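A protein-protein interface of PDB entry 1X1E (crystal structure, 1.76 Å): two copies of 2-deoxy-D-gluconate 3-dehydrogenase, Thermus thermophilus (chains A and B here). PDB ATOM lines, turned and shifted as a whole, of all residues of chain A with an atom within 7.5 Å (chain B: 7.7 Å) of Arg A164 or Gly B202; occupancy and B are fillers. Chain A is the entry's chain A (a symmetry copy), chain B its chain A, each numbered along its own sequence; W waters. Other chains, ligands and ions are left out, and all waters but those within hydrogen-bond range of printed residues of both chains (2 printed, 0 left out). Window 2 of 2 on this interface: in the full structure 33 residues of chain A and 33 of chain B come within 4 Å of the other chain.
The backbone carbonyl oxygen (O) of Arg B203 sits at hydrogen-bond distance from the side-chain hydroxyl (OH) of Tyr A224.
O of Tyr A224 lies within hydrogen-bond range of N of Gly B234, at 2.9 Å.
O of Tyr A224 sits at hydrogen-bond distance from N of Asp B233, at 3.3 Å.
The guanidinium group (NE) of Arg A164 sits at hydrogen-bond distance from the backbone carbonyl oxygen (O) of Pro B200, 3.1 Å away.
NE of Arg A164 sits close to N of Gly B202 (3.5 Å).
SD of Met B201 lies within hydrogen-bond range of NE of Arg A168 (3.5 Å).
O of Ala A163 sits at hydrogen-bond distance from NH1 of Arg A168.
The backbone NH (N) of Met B201 is in hydrogen-bond range of the backbone carbonyl oxygen (O) of Gly B234 (3.3 Å).
The side-chain hydroxyl of Thr B196 sits at hydrogen-bond distance from the indole nitrogen of Trp B204, 3.1 Å away.
The side-chain carboxylate of Asp B233 is in hydrogen-bond range of the backbone NH of Gly B235.
Among the printed residues, merely in contact across the chains: Lys A160 with Pro B200 (3.9 Å), Ala A163 with Pro B200 (3.5 Å), Ala A163 with Met B201 (3.7 Å), Arg A164 with Met B201 (3.5 Å), Tyr A224 with Ile B199 (3.8 Å), Tyr A224 with Met B201 (3.7 Å) and Tyr A224 with Trp B204 (3.5 Å).
Of chain B, only Pro B200, Met B201 and Gly B202 come within 4 Å of Arg A164.
Gly B202 touches one residue of chain A.
Ala A163 touches two residues of chain B.
Of the printed residues of chain A, Pro B200 touches Lys A160 (3.9 Å), Ala A163 (3.5 Å) and Arg A164 (3.1 Å).
Printed residues of chain A within 4 Å of Ile B199: Tyr A224 (3.8 Å).
The nearest residue of chain A that does not touch Gly B202 is Ala A163 (5.9 Å).
Hydrophobic or aromatic side chains of chain B that line the printed part of chain A: Ile B199, Pro B200 and Met B201.
Of the 13 printed residues of chain A, 5 touch a printed residue of chain B.
Hydrophobic or aromatic side chains of chain A that line the printed part of chain B: Ala A163 and Tyr A224.
Among the printed residues, 13 pairs touch across the chains.
No position is printed for both chains.
Of the 13 pairs that touch across the chains among the printed residues, none has its exchanged pair printed and touching as well.
Water W1 bridges the backbone carbonyl oxygen of Asp B233 and the side-chain hydroxyl of Tyr A224.
Water W2 lies within hydrogen-bond range of the backbone carbonyl oxygen of Ile B199, the backbone carbonyl oxygen of Thr B196 and the guanidinium group of Arg A164.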
ATOM      1  N   GLY A 120      -3.839 -10.280   6.750  1.00  0.00           N
ATOM      2  CA  GLY A 120      -5.106  -9.825   7.303  1.00  0.00           C
ATOM      3  C   GLY A 120      -6.139  -9.513   6.234  1.00  0.00           C
ATOM      4  O   GLY A 120      -7.179  -8.908   6.516  1.00  0.00           O
ATOM      5  N   LEU A 158     -14.755 -23.184   2.878  1.00  0.00           N
ATOM      6  CA  LEU A 158     -13.591 -22.353   3.163  1.00  0.00           C
ATOM      7  C   LEU A 158     -14.017 -20.940   3.555  1.00  0.00           C
ATOM      8  O   LEU A 158     -13.417 -20.326   4.440  1.00  0.00           O
ATOM      9  CB  LEU A 158     -12.648 -22.321   1.953  1.00  0.00           C
ATOM     10  CG  LEU A 158     -12.141 -23.689   1.479  1.00  0.00           C
ATOM     11  CD1 LEU A 158     -11.095 -23.490   0.395  1.00  0.00           C
ATOM     12  CD2 LEU A 158     -11.545 -24.471   2.646  1.00  0.00           C
ATOM     13  N   ALA A 159     -15.060 -20.426   2.910  1.00  0.00           N
ATOM     14  CA  ALA A 159     -15.552 -19.093   3.235  1.00  0.00           C
ATOM     15  C   ALA A 159     -15.941 -19.039   4.716  1.00  0.00           C
ATOM     16  O   ALA A 159     -15.595 -18.095   5.427  1.00  0.00           O
ATOM     17  CB  ALA A 159     -16.758 -18.754   2.367  1.00  0.00           C
ATOM     18  N   LYS A 160     -16.657 -20.061   5.176  1.00  0.00           N
ATOM     19  CA  LYS A 160     -17.096 -20.126   6.570  1.00  0.00           C
ATOM     20  C   LYS A 160     -15.915 -20.147   7.536  1.00  0.00           C
ATOM     21  O   LYS A 160     -15.885 -19.405   8.515  1.00  0.00           O
ATOM     22  CB  LYS A 160     -17.942 -21.382   6.804  1.00  0.00           C
ATOM     23  CG  LYS A 160     -18.591 -21.436   8.178  1.00  0.00           C
ATOM     24  CD  LYS A 160     -19.137 -22.825   8.499  1.00  0.00           C
ATOM     25  CE  LYS A 160     -18.008 -23.828   8.715  1.00  0.00           C
ATOM     26  NZ  LYS A 160     -18.512 -25.164   9.143  1.00  0.00           N
ATOM     27  N   GLU A 161     -14.943 -20.999   7.247  1.00  0.00           N
ATOM     28  CA  GLU A 161     -13.772 -21.148   8.100  1.00  0.00           C
ATOM     29  C   GLU A 161     -12.794 -19.981   8.128  1.00  0.00           C
ATOM     30  O   GLU A 161     -12.234 -19.668   9.184  1.00  0.00           O
ATOM     31  CB  GLU A 161     -13.014 -22.420   7.716  1.00  0.00           C
ATOM     32  CG  GLU A 161     -13.546 -23.681   8.387  1.00  0.00           C
ATOM     33  CD  GLU A 161     -12.932 -24.951   7.825  1.00  0.00           C
ATOM     34  OE1 GLU A 161     -11.754 -24.913   7.408  1.00  0.00           O
ATOM     35  OE2 GLU A 161     -13.625 -25.992   7.816  1.00  0.00           O
ATOM     36  N   TRP A 162     -12.604 -19.321   6.991  1.00  0.00           N
ATOM     37  CA  TRP A 162     -11.635 -18.233   6.921  1.00  0.00           C
ATOM     38  C   TRP A 162     -12.148 -16.795   6.982  1.00  0.00           C
ATOM     39  O   TRP A 162     -11.349 -15.852   6.930  1.00  0.00           O
ATOM     40  CB  TRP A 162     -10.774 -18.410   5.666  1.00  0.00           C
ATOM     41  CG  TRP A 162     -10.081 -19.744   5.601  1.00  0.00           C
ATOM     42  CD1 TRP A 162      -9.791 -20.572   6.654  1.00  0.00           C
ATOM     43  CD2 TRP A 162      -9.550 -20.382   4.434  1.00  0.00           C
ATOM     44  NE1 TRP A 162      -9.114 -21.682   6.212  1.00  0.00           N
ATOM     45  CE2 TRP A 162      -8.949 -21.592   4.855  1.00  0.00           C
ATOM     46  CE3 TRP A 162      -9.516 -20.051   3.072  1.00  0.00           C
ATOM     47  CZ2 TRP A 162      -8.325 -22.469   3.961  1.00  0.00           C
ATOM     48  CZ3 TRP A 162      -8.893 -20.926   2.185  1.00  0.00           C
ATOM     49  CH2 TRP A 162      -8.307 -22.122   2.637  1.00  0.00           C
ATOM     50  N   ALA A 163     -13.460 -16.625   7.109  1.00  0.00           N
ATOM     51  CA  ALA A 163     -14.060 -15.296   7.161  1.00  0.00           C
ATOM     52  C   ALA A 163     -13.449 -14.368   8.204  1.00  0.00           C
ATOM     53  O   ALA A 163     -13.174 -13.205   7.914  1.00  0.00           O
ATOM     54  CB  ALA A 163     -15.563 -15.413   7.402  1.00  0.00           C
ATOM     55  N   ARG A 164     -13.240 -14.875   9.416  1.00  0.00           N
ATOM     56  CA  ARG A 164     -12.675 -14.063  10.492  1.00  0.00           C
ATOM     57  C   ARG A 164     -11.200 -13.714  10.287  1.00  0.00           C
ATOM     58  O   ARG A 164     -10.667 -12.846  10.977  1.00  0.00           O
ATOM     59  CB  ARG A 164     -12.842 -14.775  11.835  1.00  0.00           C
ATOM     60  CG  ARG A 164     -14.283 -14.946  12.283  1.00  0.00           C
ATOM     61  CD  ARG A 164     -14.943 -13.609  12.574  1.00  0.00           C
ATOM     62  NE  ARG A 164     -16.236 -13.784  13.233  1.00  0.00           N
ATOM     63  CZ  ARG A 164     -16.399 -14.398  14.403  1.00  0.00           C
ATOM     64  NH1 ARG A 164     -15.350 -14.899  15.044  1.00  0.00           N
ATOM     65  NH2 ARG A 164     -17.611 -14.511  14.934  1.00  0.00           N
ATOM     66  N   LEU A 165     -10.549 -14.381   9.338  1.00  0.00           N
ATOM     67  CA  LEU A 165      -9.135 -14.129   9.052  1.00  0.00           C
ATOM     68  C   LEU A 165      -8.954 -13.017   8.016  1.00  0.00           C
ATOM     69  O   LEU A 165      -7.826 -12.626   7.703  1.00  0.00           O
ATOM     70  CB  LEU A 165      -8.467 -15.409   8.536  1.00  0.00           C
ATOM     71  CG  LEU A 165      -8.579 -16.676   9.393  1.00  0.00           C
ATOM     72  CD1 LEU A 165      -7.985 -17.850   8.627  1.00  0.00           C
ATOM     73  CD2 LEU A 165      -7.869 -16.483  10.726  1.00  0.00           C
ATOM     74  N   GLY A 166     -10.067 -12.516   7.482  1.00  0.00           N
ATOM     75  CA  GLY A 166     -10.015 -11.459   6.485  1.00  0.00           C
ATOM     76  C   GLY A 166     -10.036 -11.990   5.060  1.00  0.00           C
ATOM     77  O   GLY A 166      -9.823 -11.251   4.101  1.00  0.00           O
ATOM     78  N   ILE A 167     -10.305 -13.282   4.924  1.00  0.00           N
ATOM     79  CA  ILE A 167     -10.345 -13.930   3.622  1.00  0.00           C
ATOM     80  C   ILE A 167     -11.778 -14.115   3.106  1.00  0.00           C
ATOM     81  O   ILE A 167     -12.652 -14.553   3.843  1.00  0.00           O
ATOM     82  CB  ILE A 167      -9.665 -15.319   3.711  1.00  0.00           C
ATOM     83  CG1 ILE A 167      -8.248 -15.166   4.271  1.00  0.00           C
ATOM     84  CG2 ILE A 167      -9.639 -15.988   2.345  1.00  0.00           C
ATOM     85  CD1 ILE A 167      -7.477 -16.483   4.369  1.00  0.00           C
ATOM     86  N   ARG A 168     -12.010 -13.767   1.841  1.00  0.00           N
ATOM     87  CA  ARG A 168     -13.318 -13.951   1.217  1.00  0.00           C
ATOM     88  C   ARG A 168     -13.076 -15.003   0.141  1.00  0.00           C
ATOM     89  O   ARG A 168     -12.070 -14.951  -0.567  1.00  0.00           O
ATOM     90  CB  ARG A 168     -13.822 -12.656   0.573  1.00  0.00           C
ATOM     91  CG  ARG A 168     -13.802 -11.456   1.497  1.00  0.00           C
ATOM     92  CD  ARG A 168     -14.673 -11.664   2.725  1.00  0.00           C
ATOM     93  NE  ARG A 168     -14.477 -10.599   3.706  1.00  0.00           N
ATOM     94  CZ  ARG A 168     -13.916 -10.781   4.897  1.00  0.00           C
ATOM     95  NH1 ARG A 168     -13.495 -11.985   5.255  1.00  0.00           N
ATOM     96  NH2 ARG A 168     -13.785  -9.758   5.733  1.00  0.00           N
ATOM     97  N   TYR A 224     -17.864  -7.803   1.788  1.00  0.00           N
ATOM     98  CA  TYR A 224     -18.931  -8.511   2.501  1.00  0.00           C
ATOM     99  C   TYR A 224     -19.572  -9.596   1.619  1.00  0.00           C
ATOM    100  O   TYR A 224     -20.686 -10.050   1.880  1.00  0.00           O
ATOM    101  CB  TYR A 224     -20.004  -7.514   2.969  1.00  0.00           C
ATOM    102  CG  TYR A 224     -20.789  -7.961   4.189  1.00  0.00           C
ATOM    103  CD1 TYR A 224     -20.222  -7.917   5.465  1.00  0.00           C
ATOM    104  CD2 TYR A 224     -22.095  -8.433   4.067  1.00  0.00           C
ATOM    105  CE1 TYR A 224     -20.937  -8.336   6.594  1.00  0.00           C
ATOM    106  CE2 TYR A 224     -22.820  -8.856   5.186  1.00  0.00           C
ATOM    107  CZ  TYR A 224     -22.234  -8.806   6.445  1.00  0.00           C
ATOM    108  OH  TYR A 224     -22.945  -9.231   7.547  1.00  0.00           O
ATOM    109  N   TYR B 192     -30.914 -10.918  17.431  1.00  0.00           N
ATOM    110  CA  TYR B 192     -29.586 -10.547  16.954  1.00  0.00           C
ATOM    111  C   TYR B 192     -28.517 -11.615  17.167  1.00  0.00           C
ATOM    112  O   TYR B 192     -27.718 -11.886  16.269  1.00  0.00           O
ATOM    113  CB  TYR B 192     -29.145  -9.232  17.608  1.00  0.00           C
ATOM    114  CG  TYR B 192     -27.747  -8.797  17.226  1.00  0.00           C
ATOM    115  CD1 TYR B 192     -26.637  -9.233  17.948  1.00  0.00           C
ATOM    116  CD2 TYR B 192     -27.533  -7.977  16.117  1.00  0.00           C
ATOM    117  CE1 TYR B 192     -25.346  -8.866  17.577  1.00  0.00           C
ATOM    118  CE2 TYR B 192     -26.246  -7.605  15.736  1.00  0.00           C
ATOM    119  CZ  TYR B 192     -25.157  -8.053  16.469  1.00  0.00           C
ATOM    120  OH  TYR B 192     -23.882  -7.693  16.090  1.00  0.00           O
ATOM    121  N   THR B 196     -26.515 -13.437  14.084  1.00  0.00           N
ATOM    122  CA  THR B 196     -25.101 -13.098  13.990  1.00  0.00           C
ATOM    123  C   THR B 196     -24.187 -14.311  14.143  1.00  0.00           C
ATOM    124  O   THR B 196     -23.110 -14.363  13.548  1.00  0.00           O
ATOM    125  CB  THR B 196     -24.738 -12.035  15.038  1.00  0.00           C
ATOM    126  OG1 THR B 196     -25.673 -10.954  14.944  1.00  0.00           O
ATOM    127  CG2 THR B 196     -23.338 -11.492  14.792  1.00  0.00           C
ATOM    128  N   ALA B 197     -24.621 -15.291  14.928  1.00  0.00           N
ATOM    129  CA  ALA B 197     -23.836 -16.502  15.141  1.00  0.00           C
ATOM    130  C   ALA B 197     -23.671 -17.269  13.834  1.00  0.00           C
ATOM    131  O   ALA B 197     -22.726 -18.042  13.675  1.00  0.00           O
ATOM    132  CB  ALA B 197     -24.517 -17.391  16.179  1.00  0.00           C
ATOM    133  N   ARG B 198     -24.597 -17.047  12.905  1.00  0.00           N
ATOM    134  CA  ARG B 198     -24.577 -17.721  11.612  1.00  0.00           C
ATOM    135  C   ARG B 198     -23.853 -16.918  10.533  1.00  0.00           C
ATOM    136  O   ARG B 198     -23.773 -17.350   9.380  1.00  0.00           O
ATOM    137  CB  ARG B 198     -26.006 -18.019  11.157  1.00  0.00           C
ATOM    138  CG  ARG B 198     -26.742 -19.004  12.053  1.00  0.00           C
ATOM    139  CD  ARG B 198     -28.221 -19.048  11.712  1.00  0.00           C
ATOM    140  NE  ARG B 198     -28.459 -19.460  10.331  1.00  0.00           N
ATOM    141  CZ  ARG B 198     -29.653 -19.469   9.748  1.00  0.00           C
ATOM    142  NH1 ARG B 198     -30.726 -19.082  10.426  1.00  0.00           N
ATOM    143  NH2 ARG B 198     -29.780 -19.873   8.489  1.00  0.00           N
ATOM    144  N   ILE B 199     -23.336 -15.749  10.904  1.00  0.00           N
ATOM    145  CA  ILE B 199     -22.597 -14.911   9.958  1.00  0.00           C
ATOM    146  C   ILE B 199     -21.108 -15.137  10.197  1.00  0.00           C
ATOM    147  O   ILE B 199     -20.561 -14.675  11.198  1.00  0.00           O
ATOM    148  CB  ILE B 199     -22.898 -13.404  10.161  1.00  0.00           C
ATOM    149  CG1 ILE B 199     -24.403 -13.144  10.043  1.00  0.00           C
ATOM    150  CG2 ILE B 199     -22.147 -12.580   9.115  1.00  0.00           C
ATOM    151  CD1 ILE B 199     -24.811 -11.692  10.314  1.00  0.00           C
ATOM    152  N   PRO B 200     -20.435 -15.861   9.284  1.00  0.00           N
ATOM    153  CA  PRO B 200     -19.003 -16.164   9.374  1.00  0.00           C
ATOM    154  C   PRO B 200     -18.141 -14.946   9.697  1.00  0.00           C
ATOM    155  O   PRO B 200     -17.240 -15.023  10.533  1.00  0.00           O
ATOM    156  CB  PRO B 200     -18.695 -16.755   8.003  1.00  0.00           C
ATOM    157  CG  PRO B 200     -19.956 -17.503   7.690  1.00  0.00           C
ATOM    158  CD  PRO B 200     -21.035 -16.522   8.109  1.00  0.00           C
ATOM    159  N   MET B 201     -18.422 -13.824   9.042  1.00  0.00           N
ATOM    160  CA  MET B 201     -17.659 -12.604   9.277  1.00  0.00           C
ATOM    161  C   MET B 201     -17.887 -12.019  10.676  1.00  0.00           C
ATOM    162  O   MET B 201     -17.172 -11.113  11.104  1.00  0.00           O
ATOM    163  CB  MET B 201     -17.965 -11.572   8.186  1.00  0.00           C
ATOM    164  CG  MET B 201     -17.227 -11.876   6.876  1.00  0.00           C
ATOM    165  SD  MET B 201     -17.498 -10.666   5.562  1.00  0.00           S
ATOM    166  CE  MET B 201     -16.907  -9.168   6.365  1.00  0.00           C
ATOM    167  N   GLY B 202     -18.888 -12.545  11.378  1.00  0.00           N
ATOM    168  CA  GLY B 202     -19.164 -12.114  12.739  1.00  0.00           C
ATOM    169  C   GLY B 202     -19.695 -10.715  12.972  1.00  0.00           C
ATOM    170  O   GLY B 202     -19.701 -10.234  14.107  1.00  0.00           O
ATOM    171  N   ARG B 203     -20.150 -10.058  11.914  1.00  0.00           N
ATOM    172  CA  ARG B 203     -20.683  -8.710  12.049  1.00  0.00           C
ATOM    173  C   ARG B 203     -21.707  -8.438  10.963  1.00  0.00           C
ATOM    174  O   ARG B 203     -21.752  -9.139   9.957  1.00  0.00           O
ATOM    175  CB  ARG B 203     -19.558  -7.678  11.938  1.00  0.00           C
ATOM    176  CG  ARG B 203     -18.917  -7.591  10.553  1.00  0.00           C
ATOM    177  CD  ARG B 203     -17.841  -6.506  10.506  1.00  0.00           C
ATOM    178  NE  ARG B 203     -17.143  -6.467   9.222  1.00  0.00           N
ATOM    179  CZ  ARG B 203     -17.627  -5.914   8.113  1.00  0.00           C
ATOM    180  NH1 ARG B 203     -18.822  -5.344   8.117  1.00  0.00           N
ATOM    181  NH2 ARG B 203     -16.914  -5.937   6.994  1.00  0.00           N
ATOM    182  N   TRP B 204     -22.532  -7.423  11.184  1.00  0.00           N
ATOM    183  CA  TRP B 204     -23.536  -7.020  10.211  1.00  0.00           C
ATOM    184  C   TRP B 204     -22.834  -6.085   9.235  1.00  0.00           C
ATOM    185  O   TRP B 204     -21.791  -5.524   9.559  1.00  0.00           O
ATOM    186  CB  TRP B 204     -24.685  -6.296  10.913  1.00  0.00           C
ATOM    187  CG  TRP B 204     -25.642  -7.235  11.588  1.00  0.00           C
ATOM    188  CD1 TRP B 204     -25.328  -8.318  12.359  1.00  0.00           C
ATOM    189  CD2 TRP B 204     -27.070  -7.176  11.539  1.00  0.00           C
ATOM    190  NE1 TRP B 204     -26.474  -8.941  12.791  1.00  0.00           N
ATOM    191  CE2 TRP B 204     -27.558  -8.260  12.301  1.00  0.00           C
ATOM    192  CE3 TRP B 204     -27.989  -6.311  10.926  1.00  0.00           C
ATOM    193  CZ2 TRP B 204     -28.927  -8.504  12.467  1.00  0.00           C
ATOM    194  CZ3 TRP B 204     -29.351  -6.554  11.092  1.00  0.00           C
ATOM    195  CH2 TRP B 204     -29.803  -7.644  11.857  1.00  0.00           C
ATOM    196  N   ASP B 233     -23.759 -11.269   1.882  1.00  0.00           N
ATOM    197  CA  ASP B 233     -24.216 -11.512   3.247  1.00  0.00           C
ATOM    198  C   ASP B 233     -23.190 -11.897   4.298  1.00  0.00           C
ATOM    199  O   ASP B 233     -23.556 -12.454   5.341  1.00  0.00           O
ATOM    200  CB  ASP B 233     -25.291 -12.601   3.209  1.00  0.00           C
ATOM    201  CG  ASP B 233     -24.745 -13.944   2.747  1.00  0.00           C
ATOM    202  OD1 ASP B 233     -23.541 -14.024   2.426  1.00  0.00           O
ATOM    203  OD2 ASP B 233     -25.520 -14.920   2.708  1.00  0.00           O
ATOM    204  N   GLY B 234     -21.919 -11.625   4.033  1.00  0.00           N
ATOM    205  CA  GLY B 234     -20.894 -11.958   5.005  1.00  0.00           C
ATOM    206  C   GLY B 234     -20.768 -13.446   5.272  1.00  0.00           C
ATOM    207  O   GLY B 234     -20.165 -13.850   6.268  1.00  0.00           O
ATOM    208  N   GLY B 235     -21.339 -14.256   4.383  1.00  0.00           N
ATOM    209  CA  GLY B 235     -21.265 -15.699   4.523  1.00  0.00           C
ATOM    210  C   GLY B 235     -22.440 -16.381   5.195  1.00  0.00           C
ATOM    211  O   GLY B 235     -22.427 -17.598   5.373  1.00  0.00           O
HETATM  212  O   HOH W   1     -25.249 -10.829   6.761  1.00  0.00           O
HETATM  213  O   HOH W   2     -20.399 -15.357  13.932  1.00  0.00           O
